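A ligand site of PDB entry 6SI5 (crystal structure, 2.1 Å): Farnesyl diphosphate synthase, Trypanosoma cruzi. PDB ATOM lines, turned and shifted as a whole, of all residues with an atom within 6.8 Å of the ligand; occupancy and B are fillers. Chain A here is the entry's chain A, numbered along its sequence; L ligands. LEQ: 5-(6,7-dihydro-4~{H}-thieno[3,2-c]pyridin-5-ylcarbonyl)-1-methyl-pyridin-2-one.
An oxygen (O19) of the ligand lies within hydrogen-bond range of the side-chain amino group (NZ) of Lys 50 (2.9 Å). NH2 of Arg 53 lies within hydrogen-bond range of O6 of the ligand (3.3 Å).
The backbone carbonyl oxygen (O) of Phe 52 sits at hydrogen-bond distance from the side-chain hydroxyl (OG1) of Thr 56 (2.7 Å). The side-chain hydroxyl (OG1) of Thr 359 lies within hydrogen-bond range of the side-chain hydroxyl (OH) of Tyr 215, 2.8 Å away. The side-chain hydroxyl (OG1) of Thr 214 is in hydrogen-bond range of the guanidinium group (NE) of Arg 53 (3.1 Å). NH2 of Arg 53 lies close to NE2 of Gln 93, 3.1 Å away. The side-chain hydroxyl (OG1) of Thr 359 is in hydrogen-bond range of the backbone carbonyl oxygen (O) of Val 355. The backbone carbonyl oxygen of Thr 359 lies within hydrogen-bond range of the side-chain amide nitrogen of Gln 251 (3.1 Å).
Phe 52 touches the ligand. Thr 56 touches the ligand. CG2 of Thr 214 touches C15 of the ligand, at 3.5 Å. Tyr 215 touches the ligand. CE1 of Phe 248 touches N7 of the ligand, 3.3 Å away. Val 355 touches the ligand (CG1 to S11, 3.995 Å). O of Lys 358 touches C9 of the ligand (3.8 Å). Thr 359 touches the ligand (OG1 to C9, 3.4 Å). Ten residues have an atom within 4 Å of the ligand: Lys 50, Phe 52, Arg 53, Thr 56, Thr 214, Tyr 215, Phe 248, Val 355, Lys 358 and Thr 359. The nearest printed residue that does not touch the ligand is Pro 218 (5.5 Å).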
ATOM      1  N   LYS A  50      13.274  10.017   9.232  1.00  0.00           N
ATOM      2  CA  LYS A  50      14.620  10.571   9.075  1.00  0.00           C
ATOM      3  C   LYS A  50      15.488  10.392  10.347  1.00  0.00           C
ATOM      4  O   LYS A  50      16.701  10.589  10.293  1.00  0.00           O
ATOM      5  CB  LYS A  50      14.549  12.028   8.610  1.00  0.00           C
ATOM      6  CG  LYS A  50      13.924  12.187   7.229  1.00  0.00           C
ATOM      7  CD  LYS A  50      14.236  13.540   6.589  1.00  0.00           C
ATOM      8  CE  LYS A  50      13.736  13.631   5.170  1.00  0.00           C
ATOM      9  NZ  LYS A  50      12.241  13.633   5.099  1.00  0.00           N
ATOM     10  N   TYR A  51      14.862   9.989  11.465  1.00  0.00           N
ATOM     11  CA  TYR A  51      15.540   9.728  12.749  1.00  0.00           C
ATOM     12  C   TYR A  51      16.197  10.967  13.363  1.00  0.00           C
ATOM     13  O   TYR A  51      17.162  10.806  14.102  1.00  0.00           O
ATOM     14  CB  TYR A  51      16.553   8.543  12.658  1.00  0.00           C
ATOM     15  CG  TYR A  51      16.033   7.342  11.917  1.00  0.00           C
ATOM     16  CD1 TYR A  51      14.976   6.586  12.437  1.00  0.00           C
ATOM     17  CD2 TYR A  51      16.587   6.963  10.699  1.00  0.00           C
ATOM     18  CE1 TYR A  51      14.439   5.512  11.721  1.00  0.00           C
ATOM     19  CE2 TYR A  51      16.078   5.868   9.992  1.00  0.00           C
ATOM     20  CZ  TYR A  51      15.012   5.144  10.515  1.00  0.00           C
ATOM     21  OH  TYR A  51      14.475   4.103   9.814  1.00  0.00           O
ATOM     22  N   PHE A  52      15.663  12.167  13.121  1.00  0.00           N
ATOM     23  CA  PHE A  52      16.254  13.353  13.743  1.00  0.00           C
ATOM     24  C   PHE A  52      16.249  13.304  15.265  1.00  0.00           C
ATOM     25  O   PHE A  52      17.244  13.686  15.862  1.00  0.00           O
ATOM     26  CB  PHE A  52      15.633  14.659  13.231  1.00  0.00           C
ATOM     27  CG  PHE A  52      16.290  15.039  11.927  1.00  0.00           C
ATOM     28  CD1 PHE A  52      15.735  14.649  10.707  1.00  0.00           C
ATOM     29  CD2 PHE A  52      17.524  15.677  11.912  1.00  0.00           C
ATOM     30  CE1 PHE A  52      16.368  14.946   9.506  1.00  0.00           C
ATOM     31  CE2 PHE A  52      18.159  15.973  10.701  1.00  0.00           C
ATOM     32  CZ  PHE A  52      17.580  15.599   9.505  1.00  0.00           C
ATOM     33  N   ARG A  53      15.150  12.822  15.883  1.00  0.00           N
ATOM     34  CA  ARG A  53      15.023  12.755  17.346  1.00  0.00           C
ATOM     35  C   ARG A  53      16.045  11.826  17.963  1.00  0.00           C
ATOM     36  O   ARG A  53      16.768  12.224  18.882  1.00  0.00           O
ATOM     37  CB  ARG A  53      13.596  12.343  17.773  1.00  0.00           C
ATOM     38  CG  ARG A  53      12.525  13.409  17.473  1.00  0.00           C
ATOM     39  CD  ARG A  53      11.126  12.779  17.449  1.00  0.00           C
ATOM     40  NE  ARG A  53      10.124  13.736  16.954  1.00  0.00           N
ATOM     41  CZ  ARG A  53       9.818  13.913  15.675  1.00  0.00           C
ATOM     42  NH1 ARG A  53       8.907  14.815  15.329  1.00  0.00           N
ATOM     43  NH2 ARG A  53      10.425  13.207  14.730  1.00  0.00           N
ATOM     44  N   GLY A  54      16.115  10.596  17.441  1.00  0.00           N
ATOM     45  CA  GLY A  54      17.062   9.585  17.885  1.00  0.00           C
ATOM     46  C   GLY A  54      18.498  10.004  17.634  1.00  0.00           C
ATOM     47  O   GLY A  54      19.348   9.875  18.512  1.00  0.00           O
ATOM     48  N   THR A  56      19.732  13.041  17.359  1.00  0.00           N
ATOM     49  CA  THR A  56      20.163  14.191  18.176  1.00  0.00           C
ATOM     50  C   THR A  56      20.859  13.692  19.444  1.00  0.00           C
ATOM     51  O   THR A  56      21.836  14.294  19.875  1.00  0.00           O
ATOM     52  CB  THR A  56      19.009  15.136  18.461  1.00  0.00           C
ATOM     53  OG1 THR A  56      18.564  15.667  17.220  1.00  0.00           O
ATOM     54  CG2 THR A  56      19.411  16.296  19.385  1.00  0.00           C
ATOM     55  N   GLN A  93       7.940   7.975  19.855  1.00  0.00           N
ATOM     56  CA  GLN A  93       7.263   8.654  18.765  1.00  0.00           C
ATOM     57  C   GLN A  93       6.338   7.685  18.037  1.00  0.00           C
ATOM     58  O   GLN A  93       5.195   8.042  17.778  1.00  0.00           O
ATOM     59  CB  GLN A  93       8.245   9.269  17.773  1.00  0.00           C
ATOM     60  CG  GLN A  93       7.467  10.150  16.805  1.00  0.00           C
ATOM     61  CD  GLN A  93       8.218  10.506  15.593  1.00  0.00           C
ATOM     62  OE1 GLN A  93       9.187   9.834  15.188  1.00  0.00           O
ATOM     63  NE2 GLN A  93       7.765  11.577  14.976  1.00  0.00           N
ATOM     64  N   THR A 214      10.181  16.013  20.886  1.00  0.00           N
ATOM     65  CA  THR A 214      10.939  16.211  19.641  1.00  0.00           C
ATOM     66  C   THR A 214      12.257  16.908  19.908  1.00  0.00           C
ATOM     67  O   THR A 214      13.238  16.618  19.231  1.00  0.00           O
ATOM     68  CB  THR A 214      10.110  16.990  18.579  1.00  0.00           C
ATOM     69  OG1 THR A 214       8.916  16.270  18.297  1.00  0.00           O
ATOM     70  CG2 THR A 214      10.870  17.165  17.257  1.00  0.00           C
ATOM     71  N   TYR A 215      12.274  17.864  20.864  1.00  0.00           N
ATOM     72  CA  TYR A 215      13.482  18.635  21.088  1.00  0.00           C
ATOM     73  C   TYR A 215      14.070  18.562  22.479  1.00  0.00           C
ATOM     74  O   TYR A 215      15.279  18.391  22.602  1.00  0.00           O
ATOM     75  CB  TYR A 215      13.265  20.108  20.708  1.00  0.00           C
ATOM     76  CG  TYR A 215      13.117  20.268  19.223  1.00  0.00           C
ATOM     77  CD1 TYR A 215      14.232  20.379  18.395  1.00  0.00           C
ATOM     78  CD2 TYR A 215      11.864  20.305  18.622  1.00  0.00           C
ATOM     79  CE1 TYR A 215      14.103  20.503  17.012  1.00  0.00           C
ATOM     80  CE2 TYR A 215      11.716  20.442  17.244  1.00  0.00           C
ATOM     81  CZ  TYR A 215      12.855  20.535  16.443  1.00  0.00           C
ATOM     82  OH  TYR A 215      12.745  20.681  15.081  1.00  0.00           O
ATOM     83  N   PRO A 218      15.485  14.616  23.275  1.00  0.00           N
ATOM     84  CA  PRO A 218      16.760  14.255  22.640  1.00  0.00           C
ATOM     85  C   PRO A 218      17.970  15.016  23.186  1.00  0.00           C
ATOM     86  O   PRO A 218      18.996  14.405  23.438  1.00  0.00           O
ATOM     87  CB  PRO A 218      16.510  14.576  21.150  1.00  0.00           C
ATOM     88  CG  PRO A 218      15.083  14.525  20.977  1.00  0.00           C
ATOM     89  CD  PRO A 218      14.504  15.051  22.268  1.00  0.00           C
ATOM     90  N   ILE A 244      12.545  26.315  19.373  1.00  0.00           N
ATOM     91  CA  ILE A 244      12.801  25.590  18.114  1.00  0.00           C
ATOM     92  C   ILE A 244      11.579  24.685  17.808  1.00  0.00           C
ATOM     93  O   ILE A 244      11.162  24.597  16.651  1.00  0.00           O
ATOM     94  CB  ILE A 244      14.126  24.799  18.120  1.00  0.00           C
ATOM     95  CG1 ILE A 244      15.347  25.762  18.282  1.00  0.00           C
ATOM     96  CG2 ILE A 244      14.266  23.948  16.832  1.00  0.00           C
ATOM     97  CD1 ILE A 244      16.736  25.044  18.461  1.00  0.00           C
ATOM     98  N   PHE A 248       9.118  24.502  14.475  1.00  0.00           N
ATOM     99  CA  PHE A 248       8.968  23.241  13.756  1.00  0.00           C
ATOM    100  C   PHE A 248       7.476  22.963  13.468  1.00  0.00           C
ATOM    101  O   PHE A 248       7.124  22.649  12.330  1.00  0.00           O
ATOM    102  CB  PHE A 248       9.627  22.090  14.556  1.00  0.00           C
ATOM    103  CG  PHE A 248       9.385  20.703  14.019  1.00  0.00           C
ATOM    104  CD1 PHE A 248      10.062  20.245  12.887  1.00  0.00           C
ATOM    105  CD2 PHE A 248       8.495  19.838  14.648  1.00  0.00           C
ATOM    106  CE1 PHE A 248       9.819  18.955  12.384  1.00  0.00           C
ATOM    107  CE2 PHE A 248       8.280  18.548  14.160  1.00  0.00           C
ATOM    108  CZ  PHE A 248       8.945  18.114  13.043  1.00  0.00           C
ATOM    109  N   GLN A 251       5.930  25.281  10.765  1.00  0.00           N
ATOM    110  CA  GLN A 251       6.291  24.739   9.439  1.00  0.00           C
ATOM    111  C   GLN A 251       5.342  23.563   9.053  1.00  0.00           C
ATOM    112  O   GLN A 251       4.820  23.564   7.944  1.00  0.00           O
ATOM    113  CB  GLN A 251       7.731  24.194   9.452  1.00  0.00           C
ATOM    114  CG  GLN A 251       8.847  25.218   9.431  1.00  0.00           C
ATOM    115  CD  GLN A 251      10.166  24.475   9.540  1.00  0.00           C
ATOM    116  OE1 GLN A 251      10.462  23.807  10.543  1.00  0.00           O
ATOM    117  NE2 GLN A 251      10.990  24.548   8.505  1.00  0.00           N
ATOM    118  N   ASP A 252       5.104  22.595   9.976  1.00  0.00           N
ATOM    119  CA  ASP A 252       4.190  21.450   9.745  1.00  0.00           C
ATOM    120  C   ASP A 252       2.733  21.900   9.509  1.00  0.00           C
ATOM    121  O   ASP A 252       2.026  21.276   8.706  1.00  0.00           O
ATOM    122  CB  ASP A 252       4.234  20.421  10.892  1.00  0.00           C
ATOM    123  CG  ASP A 252       5.454  19.514  10.932  1.00  0.00           C
ATOM    124  OD1 ASP A 252       6.291  19.602   9.998  1.00  0.00           O
ATOM    125  OD2 ASP A 252       5.577  18.732  11.894  1.00  0.00           O
ATOM    126  N   VAL A 354      23.280  22.996  15.379  1.00  0.00           N
ATOM    127  CA  VAL A 354      23.033  21.960  14.367  1.00  0.00           C
ATOM    128  C   VAL A 354      21.540  21.582  14.333  1.00  0.00           C
ATOM    129  O   VAL A 354      20.944  21.473  13.262  1.00  0.00           O
ATOM    130  CB  VAL A 354      23.970  20.738  14.630  1.00  0.00           C
ATOM    131  CG1 VAL A 354      23.553  19.516  13.817  1.00  0.00           C
ATOM    132  CG2 VAL A 354      25.425  21.102  14.361  1.00  0.00           C
ATOM    133  N   VAL A 355      20.921  21.430  15.500  1.00  0.00           N
ATOM    134  CA  VAL A 355      19.485  21.133  15.627  1.00  0.00           C
ATOM    135  C   VAL A 355      18.669  22.248  14.950  1.00  0.00           C
ATOM    136  O   VAL A 355      17.728  21.958  14.202  1.00  0.00           O
ATOM    137  CB  VAL A 355      19.123  20.948  17.111  1.00  0.00           C
ATOM    138  CG1 VAL A 355      17.634  21.122  17.351  1.00  0.00           C
ATOM    139  CG2 VAL A 355      19.609  19.581  17.612  1.00  0.00           C
ATOM    140  N   TRP A 356      19.069  23.501  15.188  1.00  0.00           N
ATOM    141  CA  TRP A 356      18.422  24.665  14.604  1.00  0.00           C
ATOM    142  C   TRP A 356      18.566  24.671  13.083  1.00  0.00           C
ATOM    143  O   TRP A 356      17.563  24.864  12.393  1.00  0.00           O
ATOM    144  CB  TRP A 356      18.909  25.982  15.226  1.00  0.00           C
ATOM    145  CG  TRP A 356      18.367  27.212  14.535  1.00  0.00           C
ATOM    146  CD1 TRP A 356      19.095  28.241  14.014  1.00  0.00           C
ATOM    147  CD2 TRP A 356      16.991  27.504  14.248  1.00  0.00           C
ATOM    148  NE1 TRP A 356      18.252  29.146  13.411  1.00  0.00           N
ATOM    149  CE2 TRP A 356      16.962  28.723  13.533  1.00  0.00           C
ATOM    150  CE3 TRP A 356      15.774  26.831  14.499  1.00  0.00           C
ATOM    151  CZ2 TRP A 356      15.762  29.302  13.102  1.00  0.00           C
ATOM    152  CZ3 TRP A 356      14.586  27.407  14.060  1.00  0.00           C
ATOM    153  CH2 TRP A 356      14.590  28.641  13.390  1.00  0.00           C
ATOM    154  N   GLU A 357      19.796  24.424  12.564  1.00  0.00           N
ATOM    155  CA  GLU A 357      20.076  24.390  11.125  1.00  0.00           C
ATOM    156  C   GLU A 357      19.214  23.337  10.412  1.00  0.00           C
ATOM    157  O   GLU A 357      18.670  23.612   9.354  1.00  0.00           O
ATOM    158  CB  GLU A 357      21.575  24.119  10.852  1.00  0.00           C
ATOM    159  CG  GLU A 357      22.496  25.262  11.271  1.00  0.00           C
ATOM    160  CD  GLU A 357      23.993  24.986  11.287  1.00  0.00           C
ATOM    161  OE1 GLU A 357      24.396  23.810  11.471  1.00  0.00           O
ATOM    162  OE2 GLU A 357      24.771  25.961  11.144  1.00  0.00           O
ATOM    163  N   LYS A 358      19.060  22.137  11.021  1.00  0.00           N
ATOM    164  CA  LYS A 358      18.263  21.026  10.494  1.00  0.00           C
ATOM    165  C   LYS A 358      16.768  21.341  10.533  1.00  0.00           C
ATOM    166  O   LYS A 358      16.009  20.819   9.713  1.00  0.00           O
ATOM    167  CB  LYS A 358      18.552  19.731  11.267  1.00  0.00           C
ATOM    168  CG  LYS A 358      19.948  19.156  11.010  1.00  0.00           C
ATOM    169  CD  LYS A 358      20.390  18.313  12.213  1.00  0.00           C
ATOM    170  CE  LYS A 358      21.339  17.198  11.882  1.00  0.00           C
ATOM    171  NZ  LYS A 358      21.298  16.139  12.928  1.00  0.00           N
ATOM    172  N   THR A 359      16.351  22.183  11.487  1.00  0.00           N
ATOM    173  CA  THR A 359      14.961  22.614  11.606  1.00  0.00           C
ATOM    174  C   THR A 359      14.622  23.723  10.599  1.00  0.00           C
ATOM    175  O   THR A 359      13.601  23.644   9.914  1.00  0.00           O
ATOM    176  CB  THR A 359      14.653  23.038  13.053  1.00  0.00           C
ATOM    177  OG1 THR A 359      15.001  21.965  13.910  1.00  0.00           O
ATOM    178  CG2 THR A 359      13.187  23.446  13.246  1.00  0.00           C
ATOM    179  N   HIS A 360      15.466  24.780  10.567  1.00  0.00           N
ATOM    180  CA  HIS A 360      15.365  25.988   9.739  1.00  0.00           C
ATOM    181  C   HIS A 360      15.408  25.688   8.223  1.00  0.00           C
ATOM    182  O   HIS A 360      14.757  26.396   7.451  1.00  0.00           O
ATOM    183  CB  HIS A 360      16.468  26.963  10.166  1.00  0.00           C
ATOM    184  CG  HIS A 360      16.321  28.369   9.655  1.00  0.00           C
ATOM    185  ND1 HIS A 360      17.434  29.183   9.465  1.00  0.00           N
ATOM    186  CD2 HIS A 360      15.204  29.087   9.379  1.00  0.00           C
ATOM    187  CE1 HIS A 360      16.958  30.340   9.055  1.00  0.00           C
ATOM    188  NE2 HIS A 360      15.628  30.325   8.975  1.00  0.00           N
ATOM    189  N   LYS A 361      16.133  24.639   7.802  1.00  0.00           N
ATOM    190  CA  LYS A 361      16.248  24.200   6.406  1.00  0.00           C
ATOM    191  C   LYS A 361      14.964  23.479   5.943  1.00  0.00           C
ATOM    192  O   LYS A 361      14.512  22.538   6.599  1.00  0.00           O
ATOM    193  CB  LYS A 361      17.471  23.283   6.200  1.00  0.00           C
HETATM  194  C1  LEQ L   1       9.696  14.934   8.451  1.00  0.00           C
HETATM  195  C3  LEQ L   1      11.099  15.771  10.262  1.00  0.00           C
HETATM  196  C12 LEQ L   1      16.028  17.289  16.262  1.00  0.00           C
HETATM  197  C13 LEQ L   1      14.726  17.059  16.122  1.00  0.00           C
HETATM  198  C14 LEQ L   1      14.224  17.592  14.860  1.00  0.00           C
HETATM  199  C15 LEQ L   1      12.798  17.524  14.392  1.00  0.00           C
HETATM  200  C16 LEQ L   1      13.281  16.789   9.857  1.00  0.00           C
HETATM  201  C17 LEQ L   1      13.115  16.641   8.537  1.00  0.00           C
HETATM  202  C18 LEQ L   1      11.875  16.000   8.027  1.00  0.00           C
HETATM  203  N2  LEQ L   1      10.935  15.589   8.917  1.00  0.00           N
HETATM  204  C4  LEQ L   1      12.212  16.342  10.773  1.00  0.00           C
HETATM  205  C5  LEQ L   1      12.330  16.498  12.249  1.00  0.00           C
HETATM  206  O6  LEQ L   1      11.845  15.564  12.867  1.00  0.00           O
HETATM  207  N7  LEQ L   1      12.793  17.593  12.927  1.00  0.00           N
HETATM  208  C8  LEQ L   1      13.446  18.756  12.307  1.00  0.00           C
HETATM  209  C9  LEQ L   1      14.945  18.805  12.761  1.00  0.00           C
HETATM  210  C10 LEQ L   1      15.186  18.170  14.130  1.00  0.00           C
HETATM  211  S11 LEQ L   1      16.742  18.093  14.903  1.00  0.00           S
HETATM  212  O19 LEQ L   1      11.764  15.874   6.804  1.00  0.00           O
